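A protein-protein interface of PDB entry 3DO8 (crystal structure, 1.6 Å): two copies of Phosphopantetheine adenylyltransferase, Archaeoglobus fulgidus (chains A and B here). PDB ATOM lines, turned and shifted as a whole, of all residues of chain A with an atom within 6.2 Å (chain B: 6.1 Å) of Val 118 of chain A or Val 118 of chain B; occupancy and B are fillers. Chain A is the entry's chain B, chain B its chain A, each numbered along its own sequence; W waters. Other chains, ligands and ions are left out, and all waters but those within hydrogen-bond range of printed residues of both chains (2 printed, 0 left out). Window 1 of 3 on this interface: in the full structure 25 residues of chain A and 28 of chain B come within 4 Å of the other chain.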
ATOM      1  N   LEU A  19      24.120   7.594 -14.563  1.00  0.00           N
ATOM      2  CA  LEU A  19      25.530   7.715 -14.979  1.00  0.00           C
ATOM      3  C   LEU A  19      25.721   7.333 -16.456  1.00  0.00           C
ATOM      4  O   LEU A  19      26.326   8.079 -17.251  1.00  0.00           O
ATOM      5  CB  LEU A  19      26.390   6.827 -14.100  1.00  0.00           C
ATOM      6  CG  LEU A  19      27.881   6.849 -14.231  1.00  0.00           C
ATOM      7  CD1 LEU A  19      28.401   8.121 -13.617  1.00  0.00           C
ATOM      8  CD2 LEU A  19      28.436   5.597 -13.517  1.00  0.00           C
ATOM      9  N   VAL A  22      24.071   9.962 -18.856  1.00  0.00           N
ATOM     10  CA  VAL A  22      24.913  11.139 -19.009  1.00  0.00           C
ATOM     11  C   VAL A  22      26.159  10.804 -19.888  1.00  0.00           C
ATOM     12  O   VAL A  22      26.491  11.554 -20.824  1.00  0.00           O
ATOM     13  CB  VAL A  22      25.314  11.711 -17.625  1.00  0.00           C
ATOM     14  CG1 VAL A  22      26.408  12.760 -17.796  1.00  0.00           C
ATOM     15  CG2 VAL A  22      24.072  12.212 -16.913  1.00  0.00           C
ATOM     16  N   LEU A  26      26.999  12.451 -23.552  1.00  0.00           N
ATOM     17  CA  LEU A  26      28.249  13.176 -23.758  1.00  0.00           C
ATOM     18  C   LEU A  26      29.155  12.520 -24.782  1.00  0.00           C
ATOM     19  O   LEU A  26      29.893  13.236 -25.479  1.00  0.00           O
ATOM     20  CB  LEU A  26      29.007  13.350 -22.427  1.00  0.00           C
ATOM     21  CG  LEU A  26      28.364  14.240 -21.377  1.00  0.00           C
ATOM     22  CD1 LEU A  26      29.234  14.312 -20.098  1.00  0.00           C
ATOM     23  CD2 LEU A  26      27.983  15.604 -21.913  1.00  0.00           C
ATOM     24  N   TYR A  89      35.748  14.178 -21.159  1.00  0.00           N
ATOM     25  CA  TYR A  89      35.003  14.129 -19.915  1.00  0.00           C
ATOM     26  C   TYR A  89      35.246  12.818 -19.177  1.00  0.00           C
ATOM     27  O   TYR A  89      35.394  11.769 -19.801  1.00  0.00           O
ATOM     28  CB  TYR A  89      33.505  14.237 -20.192  1.00  0.00           C
ATOM     29  CG  TYR A  89      33.058  15.590 -20.724  1.00  0.00           C
ATOM     30  CD1 TYR A  89      33.136  16.725 -19.932  1.00  0.00           C
ATOM     31  CD2 TYR A  89      32.523  15.732 -22.016  1.00  0.00           C
ATOM     32  CE1 TYR A  89      32.701  17.946 -20.377  1.00  0.00           C
ATOM     33  CE2 TYR A  89      32.119  16.964 -22.482  1.00  0.00           C
ATOM     34  CZ  TYR A  89      32.191  18.077 -21.651  1.00  0.00           C
ATOM     35  OH  TYR A  89      31.792  19.335 -22.120  1.00  0.00           O
ATOM     36  N   LEU A  90      35.260  12.904 -17.848  1.00  0.00           N
ATOM     37  CA  LEU A  90      35.334  11.720 -16.974  1.00  0.00           C
ATOM     38  C   LEU A  90      34.029  11.745 -16.202  1.00  0.00           C
ATOM     39  O   LEU A  90      33.810  12.645 -15.387  1.00  0.00           O
ATOM     40  CB  LEU A  90      36.522  11.814 -16.031  1.00  0.00           C
ATOM     41  CG  LEU A  90      36.701  10.718 -14.983  1.00  0.00           C
ATOM     42  CD1 LEU A  90      36.432   9.330 -15.513  1.00  0.00           C
ATOM     43  CD2 LEU A  90      38.107  10.800 -14.359  1.00  0.00           C
ATOM     44  N   VAL A  91      33.159  10.794 -16.491  1.00  0.00           N
ATOM     45  CA  VAL A  91      31.821  10.748 -15.917  1.00  0.00           C
ATOM     46  C   VAL A  91      31.816   9.777 -14.736  1.00  0.00           C
ATOM     47  O   VAL A  91      32.137   8.604 -14.881  1.00  0.00           O
ATOM     48  CB  VAL A  91      30.755  10.345 -16.971  1.00  0.00           C
ATOM     49  CG1 VAL A  91      29.366  10.309 -16.346  1.00  0.00           C
ATOM     50  CG2 VAL A  91      30.774  11.327 -18.140  1.00  0.00           C
ATOM     51  N   VAL A  92      31.469  10.292 -13.561  1.00  0.00           N
ATOM     52  CA  VAL A  92      31.610   9.599 -12.306  1.00  0.00           C
ATOM     53  C   VAL A  92      30.360   9.770 -11.446  1.00  0.00           C
ATOM     54  O   VAL A  92      29.524  10.628 -11.699  1.00  0.00           O
ATOM     55  CB  VAL A  92      32.849  10.102 -11.539  1.00  0.00           C
ATOM     56  CG1 VAL A  92      34.086   9.835 -12.392  1.00  0.00           C
ATOM     57  CG2 VAL A  92      32.754  11.577 -11.138  1.00  0.00           C
ATOM     58  N   SER A  93      30.294   8.949 -10.402  1.00  0.00           N
ATOM     59  CA  SER A  93      29.212   8.966  -9.413  1.00  0.00           C
ATOM     60  C   SER A  93      29.822   9.407  -8.079  1.00  0.00           C
ATOM     61  O   SER A  93      31.030   9.547  -7.973  1.00  0.00           O
ATOM     62  CB  SER A  93      28.652   7.567  -9.276  1.00  0.00           C
ATOM     63  OG  SER A  93      29.609   6.793  -8.568  1.00  0.00           O
ATOM     64  N   THR A 116      37.925  17.167 -17.649  1.00  0.00           N
ATOM     65  CA  THR A 116      36.766  17.717 -16.940  1.00  0.00           C
ATOM     66  C   THR A 116      35.962  16.580 -16.329  1.00  0.00           C
ATOM     67  O   THR A 116      35.506  15.682 -17.037  1.00  0.00           O
ATOM     68  CB  THR A 116      35.873  18.516 -17.899  1.00  0.00           C
ATOM     69  OG1 THR A 116      36.627  19.584 -18.510  1.00  0.00           O
ATOM     70  CG2 THR A 116      34.651  19.102 -17.184  1.00  0.00           C
ATOM     71  N   ILE A 117      35.805  16.615 -15.019  1.00  0.00           N
ATOM     72  CA  ILE A 117      35.008  15.625 -14.284  1.00  0.00           C
ATOM     73  C   ILE A 117      33.538  16.042 -14.242  1.00  0.00           C
ATOM     74  O   ILE A 117      33.215  17.209 -13.982  1.00  0.00           O
ATOM     75  CB  ILE A 117      35.527  15.432 -12.863  1.00  0.00           C
ATOM     76  CG1 ILE A 117      36.968  14.919 -12.888  1.00  0.00           C
ATOM     77  CG2 ILE A 117      34.579  14.526 -12.029  1.00  0.00           C
ATOM     78  CD1 ILE A 117      37.623  14.982 -11.521  1.00  0.00           C
ATOM     79  N   VAL A 118      32.674  15.078 -14.533  1.00  0.00           N
ATOM     80  CA  VAL A 118      31.213  15.289 -14.553  1.00  0.00           C
ATOM     81  C   VAL A 118      30.655  14.288 -13.566  1.00  0.00           C
ATOM     82  O   VAL A 118      30.686  13.073 -13.799  1.00  0.00           O
ATOM     83  CB  VAL A 118      30.622  15.067 -15.955  1.00  0.00           C
ATOM     84  CG1 VAL A 118      29.107  15.188 -15.954  1.00  0.00           C
ATOM     85  CG2 VAL A 118      31.263  16.056 -16.982  1.00  0.00           C
ATOM     86  N   LYS A 119      30.180  14.793 -12.438  1.00  0.00           N
ATOM     87  CA  LYS A 119      29.696  13.958 -11.346  1.00  0.00           C
ATOM     88  C   LYS A 119      28.181  13.924 -11.399  1.00  0.00           C
ATOM     89  O   LYS A 119      27.501  14.976 -11.335  1.00  0.00           O
ATOM     90  CB  LYS A 119      30.153  14.511  -9.994  1.00  0.00           C
ATOM     91  CG  LYS A 119      29.735  13.691  -8.759  1.00  0.00           C
ATOM     92  CD  LYS A 119      30.003  14.520  -7.482  1.00  0.00           C
ATOM     93  CE  LYS A 119      29.612  13.801  -6.239  1.00  0.00           C
ATOM     94  NZ  LYS A 119      29.084  14.813  -5.273  1.00  0.00           N
ATOM     95  N   VAL A 120      27.661  12.707 -11.557  1.00  0.00           N
ATOM     96  CA  VAL A 120      26.211  12.504 -11.648  1.00  0.00           C
ATOM     97  C   VAL A 120      25.761  12.031 -10.268  1.00  0.00           C
ATOM     98  O   VAL A 120      26.050  10.897  -9.885  1.00  0.00           O
ATOM     99  CB  VAL A 120      25.846  11.491 -12.774  1.00  0.00           C
ATOM    100  CG1 VAL A 120      24.336  11.320 -12.879  1.00  0.00           C
ATOM    101  CG2 VAL A 120      26.463  11.928 -14.093  1.00  0.00           C
ATOM    102  N   ASP A 121      25.075  12.909  -9.540  1.00  0.00           N
ATOM    103  CA  ASP A 121      24.679  12.631  -8.146  1.00  0.00           C
ATOM    104  C   ASP A 121      23.532  11.660  -8.108  1.00  0.00           C
ATOM    105  O   ASP A 121      22.524  11.860  -8.752  1.00  0.00           O
ATOM    106  CB  ASP A 121      24.225  13.915  -7.438  1.00  0.00           C
ATOM    107  CG  ASP A 121      25.296  14.552  -6.595  1.00  0.00           C
ATOM    108  OD1 ASP A 121      26.475  14.134  -6.664  1.00  0.00           O
ATOM    109  OD2 ASP A 121      24.952  15.471  -5.814  1.00  0.00           O
ATOM    110  N   VAL B  22      27.909  20.593 -21.718  1.00  0.00           N
ATOM    111  CA  VAL B  22      27.304  19.442 -21.028  1.00  0.00           C
ATOM    112  C   VAL B  22      25.767  19.579 -21.098  1.00  0.00           C
ATOM    113  O   VAL B  22      25.072  18.637 -21.430  1.00  0.00           O
ATOM    114  CB  VAL B  22      27.823  19.298 -19.555  1.00  0.00           C
ATOM    115  CG1 VAL B  22      26.965  18.320 -18.760  1.00  0.00           C
ATOM    116  CG2 VAL B  22      29.308  18.931 -19.539  1.00  0.00           C
ATOM    117  N   LEU B  26      23.200  17.020 -23.031  1.00  0.00           N
ATOM    118  CA  LEU B  26      22.163  16.314 -22.288  1.00  0.00           C
ATOM    119  C   LEU B  26      20.774  16.599 -22.810  1.00  0.00           C
ATOM    120  O   LEU B  26      19.939  15.689 -22.831  1.00  0.00           O
ATOM    121  CB  LEU B  26      22.194  16.669 -20.786  1.00  0.00           C
ATOM    122  CG  LEU B  26      23.377  16.125 -19.999  1.00  0.00           C
ATOM    123  CD1 LEU B  26      23.361  16.682 -18.549  1.00  0.00           C
ATOM    124  CD2 LEU B  26      23.418  14.594 -20.011  1.00  0.00           C
ATOM    125  N   TYR B  89      17.568  17.078 -15.480  1.00  0.00           N
ATOM    126  CA  TYR B  89      18.947  17.315 -15.057  1.00  0.00           C
ATOM    127  C   TYR B  89      19.091  18.803 -14.705  1.00  0.00           C
ATOM    128  O   TYR B  89      18.494  19.663 -15.362  1.00  0.00           O
ATOM    129  CB  TYR B  89      19.925  17.002 -16.209  1.00  0.00           C
ATOM    130  CG  TYR B  89      20.037  15.526 -16.540  1.00  0.00           C
ATOM    131  CD1 TYR B  89      20.565  14.635 -15.623  1.00  0.00           C
ATOM    132  CD2 TYR B  89      19.611  15.030 -17.771  1.00  0.00           C
ATOM    133  CE1 TYR B  89      20.694  13.303 -15.913  1.00  0.00           C
ATOM    134  CE2 TYR B  89      19.710  13.675 -18.064  1.00  0.00           C
ATOM    135  CZ  TYR B  89      20.264  12.819 -17.121  1.00  0.00           C
ATOM    136  OH  TYR B  89      20.419  11.450 -17.345  1.00  0.00           O
ATOM    137  N   LEU B  90      19.941  19.063 -13.721  1.00  0.00           N
ATOM    138  CA  LEU B  90      20.355  20.400 -13.342  1.00  0.00           C
ATOM    139  C   LEU B  90      21.874  20.397 -13.385  1.00  0.00           C
ATOM    140  O   LEU B  90      22.526  19.661 -12.621  1.00  0.00           O
ATOM    141  CB  LEU B  90      19.873  20.721 -11.927  1.00  0.00           C
ATOM    142  CG  LEU B  90      20.324  22.040 -11.246  1.00  0.00           C
ATOM    143  CD1 LEU B  90      20.145  23.307 -12.094  1.00  0.00           C
ATOM    144  CD2 LEU B  90      19.650  22.167  -9.835  1.00  0.00           C
ATOM    145  N   VAL B  91      22.422  21.163 -14.316  1.00  0.00           N
ATOM    146  CA  VAL B  91      23.848  21.206 -14.585  1.00  0.00           C
ATOM    147  C   VAL B  91      24.428  22.394 -13.824  1.00  0.00           C
ATOM    148  O   VAL B  91      23.971  23.526 -14.005  1.00  0.00           O
ATOM    149  CB  VAL B  91      24.170  21.342 -16.097  1.00  0.00           C
ATOM    150  CG1 VAL B  91      25.703  21.571 -16.281  1.00  0.00           C
ATOM    151  CG2 VAL B  91      23.690  20.094 -16.824  1.00  0.00           C
ATOM    152  N   VAL B  92      25.421  22.104 -12.979  1.00  0.00           N
ATOM    153  CA  VAL B  92      26.003  23.080 -12.067  1.00  0.00           C
ATOM    154  C   VAL B  92      27.522  22.968 -12.014  1.00  0.00           C
ATOM    155  O   VAL B  92      28.089  22.019 -12.476  1.00  0.00           O
ATOM    156  CB  VAL B  92      25.414  22.932 -10.628  1.00  0.00           C
ATOM    157  CG1 VAL B  92      23.941  23.266 -10.671  1.00  0.00           C
ATOM    158  CG2 VAL B  92      25.661  21.568 -10.061  1.00  0.00           C
ATOM    159  N   SER B  93      28.151  24.002 -11.477  1.00  0.00           N
ATOM    160  CA  SER B  93      29.584  24.045 -11.268  1.00  0.00           C
ATOM    161  C   SER B  93      29.843  23.885  -9.783  1.00  0.00           C
ATOM    162  O   SER B  93      28.906  23.813  -8.991  1.00  0.00           O
ATOM    163  CB  SER B  93      30.118  25.386 -11.724  1.00  0.00           C
ATOM    164  OG  SER B  93      29.760  26.392 -10.816  1.00  0.00           O
ATOM    165  N   THR B 116      18.015  15.255 -11.148  1.00  0.00           N
ATOM    166  CA  THR B 116      19.379  14.694 -11.132  1.00  0.00           C
ATOM    167  C   THR B 116      20.409  15.820 -11.294  1.00  0.00           C
ATOM    168  O   THR B 116      20.420  16.491 -12.318  1.00  0.00           O
ATOM    169  CB  THR B 116      19.571  13.618 -12.209  1.00  0.00           C
ATOM    170  OG1 THR B 116      18.675  12.537 -11.928  1.00  0.00           O
ATOM    171  CG2 THR B 116      20.999  13.078 -12.174  1.00  0.00           C
ATOM    172  N   ILE B 117      21.269  15.984 -10.295  1.00  0.00           N
ATOM    173  CA  ILE B 117      22.299  17.005 -10.327  1.00  0.00           C
ATOM    174  C   ILE B 117      23.516  16.470 -11.056  1.00  0.00           C
ATOM    175  O   ILE B 117      24.045  15.358 -10.741  1.00  0.00           O
ATOM    176  CB  ILE B 117      22.689  17.488  -8.915  1.00  0.00           C
ATOM    177  CG1 ILE B 117      21.452  18.065  -8.190  1.00  0.00           C
ATOM    178  CG2 ILE B 117      23.818  18.517  -8.958  1.00  0.00           C
ATOM    179  CD1 ILE B 117      21.654  18.355  -6.707  1.00  0.00           C
ATOM    180  N   VAL B 118      23.971  17.292 -12.001  1.00  0.00           N
ATOM    181  CA  VAL B 118      25.155  17.009 -12.813  1.00  0.00           C
ATOM    182  C   VAL B 118      26.177  18.109 -12.529  1.00  0.00           C
ATOM    183  O   VAL B 118      26.011  19.244 -12.957  1.00  0.00           O
ATOM    184  CB  VAL B 118      24.800  16.915 -14.329  1.00  0.00           C
ATOM    185  CG1 VAL B 118      26.087  16.652 -15.158  1.00  0.00           C
ATOM    186  CG2 VAL B 118      23.680  15.878 -14.532  1.00  0.00           C
ATOM    187  N   LYS B 119      27.197  17.780 -11.731  1.00  0.00           N
ATOM    188  CA  LYS B 119      28.177  18.752 -11.309  1.00  0.00           C
ATOM    189  C   LYS B 119      29.361  18.669 -12.234  1.00  0.00           C
ATOM    190  O   LYS B 119      30.008  17.631 -12.354  1.00  0.00           O
ATOM    191  CB  LYS B 119      28.654  18.454  -9.895  1.00  0.00           C
ATOM    192  CG  LYS B 119      29.603  19.483  -9.338  1.00  0.00           C
ATOM    193  CD  LYS B 119      30.176  18.967  -8.041  1.00  0.00           C
ATOM    194  CE  LYS B 119      31.129  19.953  -7.407  1.00  0.00           C
ATOM    195  NZ  LYS B 119      32.423  19.276  -7.024  1.00  0.00           N
ATOM    196  N   VAL B 120      29.647  19.766 -12.893  1.00  0.00           N
ATOM    197  CA  VAL B 120      30.780  19.817 -13.824  1.00  0.00           C
ATOM    198  C   VAL B 120      31.905  20.545 -13.097  1.00  0.00           C
ATOM    199  O   VAL B 120      31.768  21.726 -12.747  1.00  0.00           O
ATOM    200  CB  VAL B 120      30.383  20.559 -15.078  1.00  0.00           C
ATOM    201  CG1 VAL B 120      31.556  20.703 -16.081  1.00  0.00           C
ATOM    202  CG2 VAL B 120      29.115  19.893 -15.700  1.00  0.00           C
ATOM    203  N   ASP B 121      33.006  19.840 -12.846  1.00  0.00           N
ATOM    204  CA  ASP B 121      34.184  20.454 -12.193  1.00  0.00           C
ATOM    205  C   ASP B 121      34.929  21.239 -13.263  1.00  0.00           C
ATOM    206  O   ASP B 121      35.776  20.736 -13.991  1.00  0.00           O
ATOM    207  CB  ASP B 121      35.064  19.400 -11.540  1.00  0.00           C
ATOM    208  CG  ASP B 121      34.592  18.986 -10.134  1.00  0.00           C
ATOM    209  OD1 ASP B 121      33.524  19.413  -9.639  1.00  0.00           O
ATOM    210  OD2 ASP B 121      35.345  18.228  -9.504  1.00  0.00           O
HETATM  211  O   HOH W   1      20.946  14.396  -7.908  1.00  0.00           O
HETATM  212  O   HOH W   2      37.483  18.446 -13.532  1.00  0.00           O
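Printed residues of chain B within 4 Å of Val 118 of chain A: Val 118 and Lys 119. Val 118 of chain B touches just these residues of chain A: Val 118 and Lys 119. Printed residues of chain B within 4 Å of Leu 26 of chain A: Val 22. Printed residues of chain A within 4 Å of Asp 121 of chain B: Thr 116 (3.8 Å) and Ile 117 (2.9 Å). Printed residues of chain A within 4 Å of Lys 119 of chain B: Ile 117, Val 118 and Lys 119. Leu 90 of chain B touches none of the printed residues of chain A. Ser 93 of chain B touches none of the printed residues of chain A. The nearest residue of chain B that does not touch Val 118 of chain A is Val 22 of chain B (4.3 Å). The nearest residue of chain A that does not touch Val 118 of chain B is Val 22 of chain A (4.4 Å). The nearest printed residue of chain A that does not touch Leu 26 of chain B is Leu 26 of chain A (5.0 Å).
Val 22 of chain A touches Leu 26 of chain B, and with the chains exchanged Leu 26 of chain A touches Val 22 of chain B. Thr 116 of chain A touches Asp 121 of chain B, and with the chains exchanged Asp 121 of chain A touches Thr 116 of chain B. Ile 117 of chain A touches Val 120 of chain B, and with the chains exchanged Val 120 of chain A touches Ile 117 of chain B. Ile 117 of chain A touches Asp 121 of chain B, and with the chains exchanged Asp 121 of chain A touches Ile 117 of chain B. Of the 18 pairs that touch across the chains among the printed residues, 18 have their exchanged pair printed and touching as well.
Water W1 bridges N of Ile 117 of chain B and O of Asp 121 of chain A. Water W2 bridges the backbone carbonyl oxygen (O) of Asp 121 of chain B (2.9 Å) and the backbone NH (N) of Ile 117 of chain A (2.9 Å).
Among the printed residues, merely in contact across the chains: Val 22 of chain A with Leu 26 of chain B (3.9 Å), Val 22 of chain A with Tyr 89 of chain B (3.7 Å), Leu 26 of chain A with Val 22 of chain B (3.997 Å), Tyr 89 of chain A with Val 22 of chain B (3.6 Å), Thr 116 of chain A with Val 120 of chain B (3.7 Å), Thr 116 of chain A with Asp 121 of chain B (3.8 Å), Ile 117 of chain A with Lys 119 of chain B (3.6 Å), Ile 117 of chain A with Val 120 of chain B (3.6 Å), Val 118 of chain A with Val 118 of chain B (3.4 Å), Val 118 of chain A with Lys 119 of chain B (3.4 Å), Lys 119 of chain A with Ile 117 of chain B (3.5 Å), Lys 119 of chain A with Val 118 of chain B (3.4 Å), Val 120 of chain A with Thr 116 of chain B (3.8 Å), Val 120 of chain A with Ile 117 of chain B (3.7 Å) and Asp 121 of chain A with Thr 116 of chain B (3.9 Å).
The backbone carbonyl oxygen of Val 92 of chain B sits at hydrogen-bond distance from the backbone NH of Val 120 of chain B, 2.8 Å away. The backbone NH (N) of Val 92 of chain B lies within hydrogen-bond range of the backbone carbonyl oxygen (O) of Val 118 of chain B (2.9 Å). N of Val 92 of chain A lies within hydrogen-bond range of O of Val 118 of chain A (2.9 Å). The backbone carbonyl oxygen (O) of Leu 90 of chain A is in hydrogen-bond range of the backbone NH (N) of Val 118 of chain A (2.8 Å). O of Thr 116 of chain A sits at hydrogen-bond distance from N of Leu 90 of chain A, 2.9 Å away. The backbone carbonyl oxygen (O) of Val 92 of chain A is in hydrogen-bond range of the backbone NH (N) of Val 120 of chain A (2.8 Å).
The backbone NH (N) of Asp 121 of chain B sits at hydrogen-bond distance from the backbone carbonyl oxygen (O) of Ile 117 of chain A, at 2.9 Å. The backbone carbonyl oxygen (O) of Ile 117 of chain B is in hydrogen-bond range of the backbone NH (N) of Asp 121 of chain A, 2.9 Å away. O of Lys 119 of chain B is in hydrogen-bond range of N of Lys 119 of chain A (2.8 Å).
Hydrophobic or aromatic side chains of chain A within 4 Å of the printed part of chain B: Val 22, Leu 26, Tyr 89, Val 118 and Val 120. Of the 13 printed residues of chain B, 9 touch a printed residue of chain A. Printed residues of chain B that touch a printed residue of chain A: Val 22, Leu 26, Tyr 89, Thr 116, Ile 117, Val 118, Lys 119, Val 120 and Asp 121. Among the printed residues, 18 pairs touch across the chains. Among the printed residues, no Asp or Glu carboxylate lies within 4 Å of a Lys or Arg side-chain nitrogen of the other chain.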
